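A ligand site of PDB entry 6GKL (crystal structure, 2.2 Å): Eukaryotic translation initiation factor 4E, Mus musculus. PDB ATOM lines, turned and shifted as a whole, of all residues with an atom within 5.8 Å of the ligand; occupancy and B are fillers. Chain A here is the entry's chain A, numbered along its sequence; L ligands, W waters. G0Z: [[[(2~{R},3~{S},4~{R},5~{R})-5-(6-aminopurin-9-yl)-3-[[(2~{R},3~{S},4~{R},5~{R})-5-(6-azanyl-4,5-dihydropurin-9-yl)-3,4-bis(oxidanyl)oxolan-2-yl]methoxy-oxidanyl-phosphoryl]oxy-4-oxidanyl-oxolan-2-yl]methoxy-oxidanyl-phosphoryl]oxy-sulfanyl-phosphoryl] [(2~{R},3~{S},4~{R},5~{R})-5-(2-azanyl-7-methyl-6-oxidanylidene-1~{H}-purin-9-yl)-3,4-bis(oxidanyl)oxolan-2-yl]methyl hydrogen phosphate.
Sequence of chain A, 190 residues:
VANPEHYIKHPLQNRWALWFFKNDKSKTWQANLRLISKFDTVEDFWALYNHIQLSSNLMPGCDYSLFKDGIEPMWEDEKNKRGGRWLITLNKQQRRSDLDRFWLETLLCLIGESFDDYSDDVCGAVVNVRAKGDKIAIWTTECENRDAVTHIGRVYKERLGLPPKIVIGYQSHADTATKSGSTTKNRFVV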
ATOM      1  N   TRP A  29     -31.030   5.826   9.718  1.00  0.00           N
ATOM      2  CA  TRP A  29     -30.779   6.316  11.059  1.00  0.00           C
ATOM      3  C   TRP A  29     -31.706   5.652  12.062  1.00  0.00           C
ATOM      4  O   TRP A  29     -31.252   5.204  13.126  1.00  0.00           O
ATOM      5  CB  TRP A  29     -30.973   7.833  11.117  1.00  0.00           C
ATOM      6  CG  TRP A  29     -30.677   8.407  12.477  1.00  0.00           C
ATOM      7  CD1 TRP A  29     -29.446   8.812  12.938  1.00  0.00           C
ATOM      8  CD2 TRP A  29     -31.600   8.613  13.567  1.00  0.00           C
ATOM      9  NE1 TRP A  29     -29.558   9.264  14.228  1.00  0.00           N
ATOM     10  CE2 TRP A  29     -30.867   9.151  14.643  1.00  0.00           C
ATOM     11  CE3 TRP A  29     -32.971   8.407  13.723  1.00  0.00           C
ATOM     12  CZ2 TRP A  29     -31.458   9.473  15.864  1.00  0.00           C
ATOM     13  CZ3 TRP A  29     -33.563   8.729  14.944  1.00  0.00           C
ATOM     14  CH2 TRP A  29     -32.795   9.262  16.006  1.00  0.00           C
ATOM     15  N   ASP A  63     -24.725   6.566  20.547  1.00  0.00           N
ATOM     16  CA  ASP A  63     -25.521   7.367  21.466  1.00  0.00           C
ATOM     17  C   ASP A  63     -26.138   6.453  22.516  1.00  0.00           C
ATOM     18  O   ASP A  63     -26.515   5.324  22.220  1.00  0.00           O
ATOM     19  CB  ASP A  63     -26.721   8.145  20.825  1.00  0.00           C
ATOM     20  CG  ASP A  63     -26.377   8.830  19.524  1.00  0.00           C
ATOM     21  OD1 ASP A  63     -25.289   9.435  19.435  1.00  0.00           O
ATOM     22  OD2 ASP A  63     -27.247   8.830  18.621  1.00  0.00           O
ATOM     23  N   PRO A  73     -36.673   8.440  21.284  1.00  0.00           N
ATOM     24  CA  PRO A  73     -35.667   9.526  21.298  1.00  0.00           C
ATOM     25  C   PRO A  73     -35.427  10.135  19.914  1.00  0.00           C
ATOM     26  O   PRO A  73     -34.300  10.180  19.413  1.00  0.00           O
ATOM     27  CB  PRO A  73     -34.402   8.837  21.835  1.00  0.00           C
ATOM     28  CG  PRO A  73     -34.618   7.373  21.676  1.00  0.00           C
ATOM     29  CD  PRO A  73     -36.068   7.106  21.396  1.00  0.00           C
ATOM     30  N   MET A  74     -36.493  10.629  19.280  1.00  0.00           N
ATOM     31  CA  MET A  74     -36.355  11.212  17.948  1.00  0.00           C
ATOM     32  C   MET A  74     -37.264  12.416  17.817  1.00  0.00           C
ATOM     33  O   MET A  74     -38.288  12.521  18.508  1.00  0.00           O
ATOM     34  CB  MET A  74     -36.660  10.177  16.841  1.00  0.00           C
ATOM     35  CG  MET A  74     -37.986   9.475  16.996  1.00  0.00           C
ATOM     36  SD  MET A  74     -38.347   8.280  15.689  1.00  0.00           S
ATOM     37  CE  MET A  74     -37.199   6.957  16.064  1.00  0.00           C
ATOM     38  N   TRP A  75     -36.893  13.331  16.913  1.00  0.00           N
ATOM     39  CA  TRP A  75     -37.675  14.555  16.715  1.00  0.00           C
ATOM     40  C   TRP A  75     -39.131  14.256  16.369  1.00  0.00           C
ATOM     41  O   TRP A  75     -40.027  15.026  16.749  1.00  0.00           O
ATOM     42  CB  TRP A  75     -37.085  15.382  15.577  1.00  0.00           C
ATOM     43  CG  TRP A  75     -35.647  15.698  15.697  1.00  0.00           C
ATOM     44  CD1 TRP A  75     -34.948  15.997  16.845  1.00  0.00           C
ATOM     45  CD2 TRP A  75     -34.700  15.766  14.630  1.00  0.00           C
ATOM     46  NE1 TRP A  75     -33.630  16.244  16.545  1.00  0.00           N
ATOM     47  CE2 TRP A  75     -33.453  16.096  15.194  1.00  0.00           C
ATOM     48  CE3 TRP A  75     -34.787  15.563  13.249  1.00  0.00           C
ATOM     49  CZ2 TRP A  75     -32.303  16.237  14.434  1.00  0.00           C
ATOM     50  CZ3 TRP A  75     -33.648  15.702  12.498  1.00  0.00           C
ATOM     51  CH2 TRP A  75     -32.425  16.033  13.089  1.00  0.00           C
ATOM     52  N   GLU A  76     -39.389  13.167  15.668  1.00  0.00           N
ATOM     53  CA  GLU A  76     -40.733  12.966  15.130  1.00  0.00           C
ATOM     54  C   GLU A  76     -41.747  12.525  16.170  1.00  0.00           C
ATOM     55  O   GLU A  76     -42.948  12.534  15.877  1.00  0.00           O
ATOM     56  CB  GLU A  76     -40.688  11.932  13.997  1.00  0.00           C
ATOM     57  CG  GLU A  76     -39.940  12.367  12.759  1.00  0.00           C
ATOM     58  CD  GLU A  76     -38.426  12.308  12.928  1.00  0.00           C
ATOM     59  OE1 GLU A  76     -37.949  11.524  13.774  1.00  0.00           O
ATOM     60  OE2 GLU A  76     -37.717  13.044  12.216  1.00  0.00           O
ATOM     61  N   ARG A  85     -33.836  21.168  23.103  1.00  0.00           N
ATOM     62  CA  ARG A  85     -32.823  20.554  23.945  1.00  0.00           C
ATOM     63  C   ARG A  85     -31.924  21.605  24.594  1.00  0.00           C
ATOM     64  O   ARG A  85     -31.559  22.596  23.963  1.00  0.00           O
ATOM     65  CB  ARG A  85     -31.965  19.559  23.155  1.00  0.00           C
ATOM     66  CG  ARG A  85     -31.091  20.181  22.059  1.00  0.00           C
ATOM     67  CD  ARG A  85     -30.235  19.137  21.364  1.00  0.00           C
ATOM     68  NE  ARG A  85     -29.468  19.730  20.279  1.00  0.00           N
ATOM     69  CZ  ARG A  85     -28.621  19.053  19.516  1.00  0.00           C
ATOM     70  NH1 ARG A  85     -28.427  17.758  19.707  1.00  0.00           N
ATOM     71  NH2 ARG A  85     -27.963  19.690  18.548  1.00  0.00           N
ATOM     72  N   ASN A 128     -24.213  12.002  22.785  1.00  0.00           N
ATOM     73  CA  ASN A 128     -23.681  11.659  21.476  1.00  0.00           C
ATOM     74  C   ASN A 128     -22.161  11.586  21.628  1.00  0.00           C
ATOM     75  O   ASN A 128     -21.537  12.578  22.017  1.00  0.00           O
ATOM     76  CB  ASN A 128     -24.015  12.709  20.424  1.00  0.00           C
ATOM     77  CG  ASN A 128     -25.518  12.958  20.264  1.00  0.00           C
ATOM     78  OD1 ASN A 128     -25.985  14.088  20.431  1.00  0.00           O
ATOM     79  ND2 ASN A 128     -26.266  11.912  19.930  1.00  0.00           N
ATOM     80  N   ARG A 130     -18.819  11.457  19.617  1.00  0.00           N
ATOM     81  CA  ARG A 130     -18.279  11.682  18.279  1.00  0.00           C
ATOM     82  C   ARG A 130     -16.810  12.085  18.332  1.00  0.00           C
ATOM     83  O   ARG A 130     -16.331  12.643  19.330  1.00  0.00           O
ATOM     84  CB  ARG A 130     -19.047  12.811  17.544  1.00  0.00           C
ATOM     85  CG  ARG A 130     -20.585  12.743  17.526  1.00  0.00           C
ATOM     86  CD  ARG A 130     -21.061  11.735  16.468  1.00  0.00           C
ATOM     87  NE  ARG A 130     -22.526  11.656  16.370  1.00  0.00           N
ATOM     88  CZ  ARG A 130     -23.296  10.871  17.126  1.00  0.00           C
ATOM     89  NH1 ARG A 130     -22.773  10.083  18.063  1.00  0.00           N
ATOM     90  NH2 ARG A 130     -24.610  10.874  16.930  1.00  0.00           N
ATOM     91  N   LYS A 132     -15.424  14.392  16.571  1.00  0.00           N
ATOM     92  CA  LYS A 132     -15.322  15.844  16.506  1.00  0.00           C
ATOM     93  C   LYS A 132     -15.589  16.496  17.858  1.00  0.00           C
ATOM     94  O   LYS A 132     -15.009  17.548  18.164  1.00  0.00           O
ATOM     95  CB  LYS A 132     -16.297  16.399  15.455  1.00  0.00           C
ATOM     96  N   GLY A 133     -16.454  15.890  18.660  1.00  0.00           N
ATOM     97  CA  GLY A 133     -16.773  16.417  19.972  1.00  0.00           C
ATOM     98  C   GLY A 133     -18.060  15.816  20.515  1.00  0.00           C
ATOM     99  O   GLY A 133     -19.074  15.785  19.805  1.00  0.00           O
ATOM    100  N   LYS A 135     -21.510  15.364  22.916  1.00  0.00           N
ATOM    101  CA  LYS A 135     -22.630  16.210  23.271  1.00  0.00           C
ATOM    102  C   LYS A 135     -23.533  15.508  24.266  1.00  0.00           C
ATOM    103  O   LYS A 135     -23.763  14.296  24.170  1.00  0.00           O
ATOM    104  CB  LYS A 135     -23.464  16.605  22.042  1.00  0.00           C
ATOM    105  CG  LYS A 135     -22.807  17.644  21.157  1.00  0.00           C
ATOM    106  CD  LYS A 135     -23.621  17.887  19.905  1.00  0.00           C
ATOM    107  CE  LYS A 135     -22.911  17.326  18.707  1.00  0.00           C
ATOM    108  NZ  LYS A 135     -23.409  17.931  17.443  1.00  0.00           N
ATOM    109  N   TRP A 139     -33.782  16.893  26.584  1.00  0.00           N
ATOM    110  CA  TRP A 139     -34.854  17.221  25.675  1.00  0.00           C
ATOM    111  C   TRP A 139     -36.102  17.524  26.502  1.00  0.00           C
ATOM    112  O   TRP A 139     -36.462  16.745  27.375  1.00  0.00           O
ATOM    113  CB  TRP A 139     -35.152  16.054  24.746  1.00  0.00           C
ATOM    114  CG  TRP A 139     -34.148  15.817  23.687  1.00  0.00           C
ATOM    115  CD1 TRP A 139     -32.812  16.148  23.704  1.00  0.00           C
ATOM    116  CD2 TRP A 139     -34.397  15.207  22.417  1.00  0.00           C
ATOM    117  NE1 TRP A 139     -32.225  15.770  22.516  1.00  0.00           N
ATOM    118  CE2 TRP A 139     -33.180  15.189  21.716  1.00  0.00           C
ATOM    119  CE3 TRP A 139     -35.539  14.660  21.817  1.00  0.00           C
ATOM    120  CZ2 TRP A 139     -33.062  14.654  20.436  1.00  0.00           C
ATOM    121  CZ3 TRP A 139     -35.425  14.136  20.544  1.00  0.00           C
ATOM    122  CH2 TRP A 139     -34.203  14.129  19.872  1.00  0.00           C
ATOM    123  N   THR A 176     -33.231  22.246  14.470  1.00  0.00           N
ATOM    124  CA  THR A 176     -32.198  21.256  14.196  1.00  0.00           C
ATOM    125  C   THR A 176     -32.568  20.381  12.999  1.00  0.00           C
ATOM    126  O   THR A 176     -31.705  20.060  12.176  1.00  0.00           O
ATOM    127  CB  THR A 176     -31.963  20.366  15.422  1.00  0.00           C
ATOM    128  OG1 THR A 176     -31.812  21.177  16.588  1.00  0.00           O
ATOM    129  CG2 THR A 176     -30.721  19.524  15.221  1.00  0.00           C
ATOM    130  N   LYS A 179     -31.774  21.432   9.542  1.00  0.00           N
ATOM    131  CA  LYS A 179     -30.333  21.509   9.314  1.00  0.00           C
ATOM    132  C   LYS A 179     -29.870  22.953   9.258  1.00  0.00           C
ATOM    133  O   LYS A 179     -29.554  23.549  10.293  1.00  0.00           O
ATOM    134  CB  LYS A 179     -29.946  20.763   8.034  1.00  0.00           C
ATOM    135  CG  LYS A 179     -30.354  19.301   8.009  1.00  0.00           C
HETATM  136  O1  G0Z L   1     -34.280  12.588  15.759  1.00  0.00           O
HETATM  137  C1  G0Z L   1     -33.846  12.268  14.522  1.00  0.00           C
HETATM  138  N1  G0Z L   1     -34.733  11.875  13.585  1.00  0.00           N
HETATM  139  C2  G0Z L   1     -34.279  11.555  12.361  1.00  0.00           C
HETATM  140  N2  G0Z L   1     -35.122  11.160  11.411  1.00  0.00           N
HETATM  141  N3  G0Z L   1     -32.973  11.635  12.099  1.00  0.00           N
HETATM  142  C3  G0Z L   1     -32.107  12.025  13.045  1.00  0.00           C
HETATM  143  C4  G0Z L   1     -32.531  12.352  14.261  1.00  0.00           C
HETATM  144  N4  G0Z L   1     -31.449  12.696  14.971  1.00  0.00           N
HETATM  145  C5  G0Z L   1     -31.329  13.145  16.384  1.00  0.00           C
HETATM  146  C6  G0Z L   1     -30.375  12.589  14.185  1.00  0.00           C
HETATM  147  N5  G0Z L   1     -30.783  12.152  13.003  1.00  0.00           N
HETATM  148  C7  G0Z L   1     -29.979  11.898  11.759  1.00  0.00           C
HETATM  149  O2  G0Z L   1     -28.612  11.725  12.098  1.00  0.00           O
HETATM  150  C8  G0Z L   1     -30.106  13.154  10.943  1.00  0.00           C
HETATM  151  O3  G0Z L   1     -30.037  12.767   9.548  1.00  0.00           O
HETATM  152  C9  G0Z L   1     -28.837  13.873  11.253  1.00  0.00           C
HETATM  153  O4  G0Z L   1     -28.504  14.755  10.195  1.00  0.00           O
HETATM  154  C10 G0Z L   1     -27.846  12.723  11.448  1.00  0.00           C
HETATM  155  C11 G0Z L   1     -26.758  13.065  12.451  1.00  0.00           C
HETATM  156  O5  G0Z L   1     -27.367  13.622  13.604  1.00  0.00           O
HETATM  157  P1  G0Z L   1     -26.652  13.792  15.044  1.00  0.00           P
HETATM  158  O6  G0Z L   1     -25.752  12.644  15.191  1.00  0.00           O
HETATM  159  O7  G0Z L   1     -27.651  14.045  16.110  1.00  0.00           O
HETATM  160  O8  G0Z L   1     -25.790  15.137  14.786  1.00  0.00           O
HETATM  161  P2  G0Z L   1     -24.283  15.153  15.342  1.00  0.00           P
HETATM  162  S1  G0Z L   1     -24.172  14.367  17.251  1.00  0.00           S
HETATM  163  O9  G0Z L   1     -23.886  16.576  15.394  1.00  0.00           O
HETATM  164  O10 G0Z L   1     -23.282  14.235  14.442  1.00  0.00           O
HETATM  165  P3  G0Z L   1     -21.883  14.740  13.825  1.00  0.00           P
HETATM  166  O11 G0Z L   1     -21.161  13.504  13.434  1.00  0.00           O
HETATM  167  O12 G0Z L   1     -21.242  15.696  14.756  1.00  0.00           O
HETATM  168  O13 G0Z L   1     -22.312  15.471  12.511  1.00  0.00           O
HETATM  169  C12 G0Z L   1     -22.687  16.839  12.543  1.00  0.00           C
HETATM  170  C13 G0Z L   1     -23.147  17.260  11.162  1.00  0.00           C
HETATM  171  O14 G0Z L   1     -22.034  16.894  10.297  1.00  0.00           O
HETATM  172  C14 G0Z L   1     -24.329  16.419  10.677  1.00  0.00           C
HETATM  173  O15 G0Z L   1     -25.123  17.210   9.809  1.00  0.00           O
HETATM  174  C15 G0Z L   1     -23.671  15.274   9.952  1.00  0.00           C
HETATM  175  O16 G0Z L   1     -24.573  14.707   8.990  1.00  0.00           O
HETATM  176  C16 G0Z L   1     -22.559  16.032   9.269  1.00  0.00           C
HETATM  177  N6  G0Z L   1     -21.449  15.123   8.896  1.00  0.00           N
HETATM  178  C17 G0Z L   1     -20.468  14.774   9.711  1.00  0.00           C
HETATM  179  N7  G0Z L   1     -19.663  13.940   9.051  1.00  0.00           N
HETATM  180  C18 G0Z L   1     -20.159  13.779   7.832  1.00  0.00           C
HETATM  181  C19 G0Z L   1     -21.275  14.510   7.737  1.00  0.00           C
HETATM  182  N8  G0Z L   1     -21.986  14.536   6.605  1.00  0.00           N
HETATM  183  C20 G0Z L   1     -21.561  13.786   5.499  1.00  0.00           C
HETATM  184  N9  G0Z L   1     -20.396  13.026   5.630  1.00  0.00           N
HETATM  185  C21 G0Z L   1     -19.737  13.058   6.792  1.00  0.00           C
HETATM  186  N10 G0Z L   1     -18.621  12.366   6.982  1.00  0.00           N
HETATM  187  P4  G0Z L   1     -26.570  17.664  10.307  1.00  0.00           P
HETATM  188  O17 G0Z L   1     -27.345  18.150   9.149  1.00  0.00           O
HETATM  189  O18 G0Z L   1     -27.136  16.606  11.181  1.00  0.00           O
HETATM  190  O19 G0Z L   1     -26.146  18.903  11.208  1.00  0.00           O
HETATM  191  O20 G0Z L   1     -25.354  23.467  12.178  1.00  0.00           O
HETATM  192  C22 G0Z L   1     -23.171  21.720  11.949  1.00  0.00           C
HETATM  193  C23 G0Z L   1     -23.745  22.447  10.737  1.00  0.00           C
HETATM  194  C24 G0Z L   1     -25.195  22.519  11.117  1.00  0.00           C
HETATM  195  C25 G0Z L   1     -25.413  21.123  11.690  1.00  0.00           C
HETATM  196  C26 G0Z L   1     -25.983  20.182  10.622  1.00  0.00           C
HETATM  197  O21 G0Z L   1     -24.099  20.636  12.125  1.00  0.00           O
HETATM  198  O22 G0Z L   1     -23.206  23.786  10.688  1.00  0.00           O
HETATM  199  N11 G0Z L   1     -21.808  21.207  11.670  1.00  0.00           N
HETATM  200  O   HOH W   1     -27.882  10.549  16.698  1.00  0.00           O
HETATM  201  O   HOH W   2     -26.173  10.203  14.136  1.00  0.00           O
HETATM  202  O   HOH W   3     -29.639  14.579  18.987  1.00  0.00           O
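The guanidinium group (NH1) of Arg 130 is in salt-bridge range of the side-chain carboxylate (OD1) of Asp 63. The side-chain carboxylate of Asp 63 lies within hydrogen-bond range of the side-chain amide nitrogen of Asn 128, 2.7 Å away. The backbone carbonyl oxygen (O) of Lys 135 is in hydrogen-bond range of the backbone NH (N) of Asn 128 (2.7 Å).
Met 74 touches the ligand (CA to O1, 3.3 Å). Lys 179 touches the ligand. Eight residues have an atom within 4 Å of the ligand: Trp 29, Met 74, Trp 75, Glu 76, Asn 128, Arg 130, Lys 135 and Lys 179. The nearest printed residue that does not touch the ligand is Pro 73 (4.4 Å).
N of Trp 75 lies within hydrogen-bond range of O1 of the ligand (3.0 Å). NH2 of Arg 130 is in salt-bridge range of O6 of the ligand (2.7 Å). N1 of the ligand lies within hydrogen-bond range of OE1 of Glu 76. A sulfur (S1) of the ligand sits close to the side-chain amide oxygen of Asn 128 (3.7 Å). An oxygen (O2) of the ligand sits close to the indole nitrogen (NE1) of Trp 29 (3.4 Å). The side-chain amino group (NZ) of Lys 135 sits at hydrogen-bond distance from an oxygen (O9) of the ligand.
Water W2 bridges an oxygen (O6) of the ligand (2.7 Å) and the guanidinium group (NH2) of Arg 130 (3.3 Å). Water W1 lies within hydrogen-bond range of the side-chain carboxylate (OD2) of Asp 63 (2.7 Å), the indole nitrogen (NE1) of Trp 29 (3.2 Å), the guanidinium group (NH2) of Arg 130 (3.3 Å) and an oxygen (O6) of the ligand (3.3 Å).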
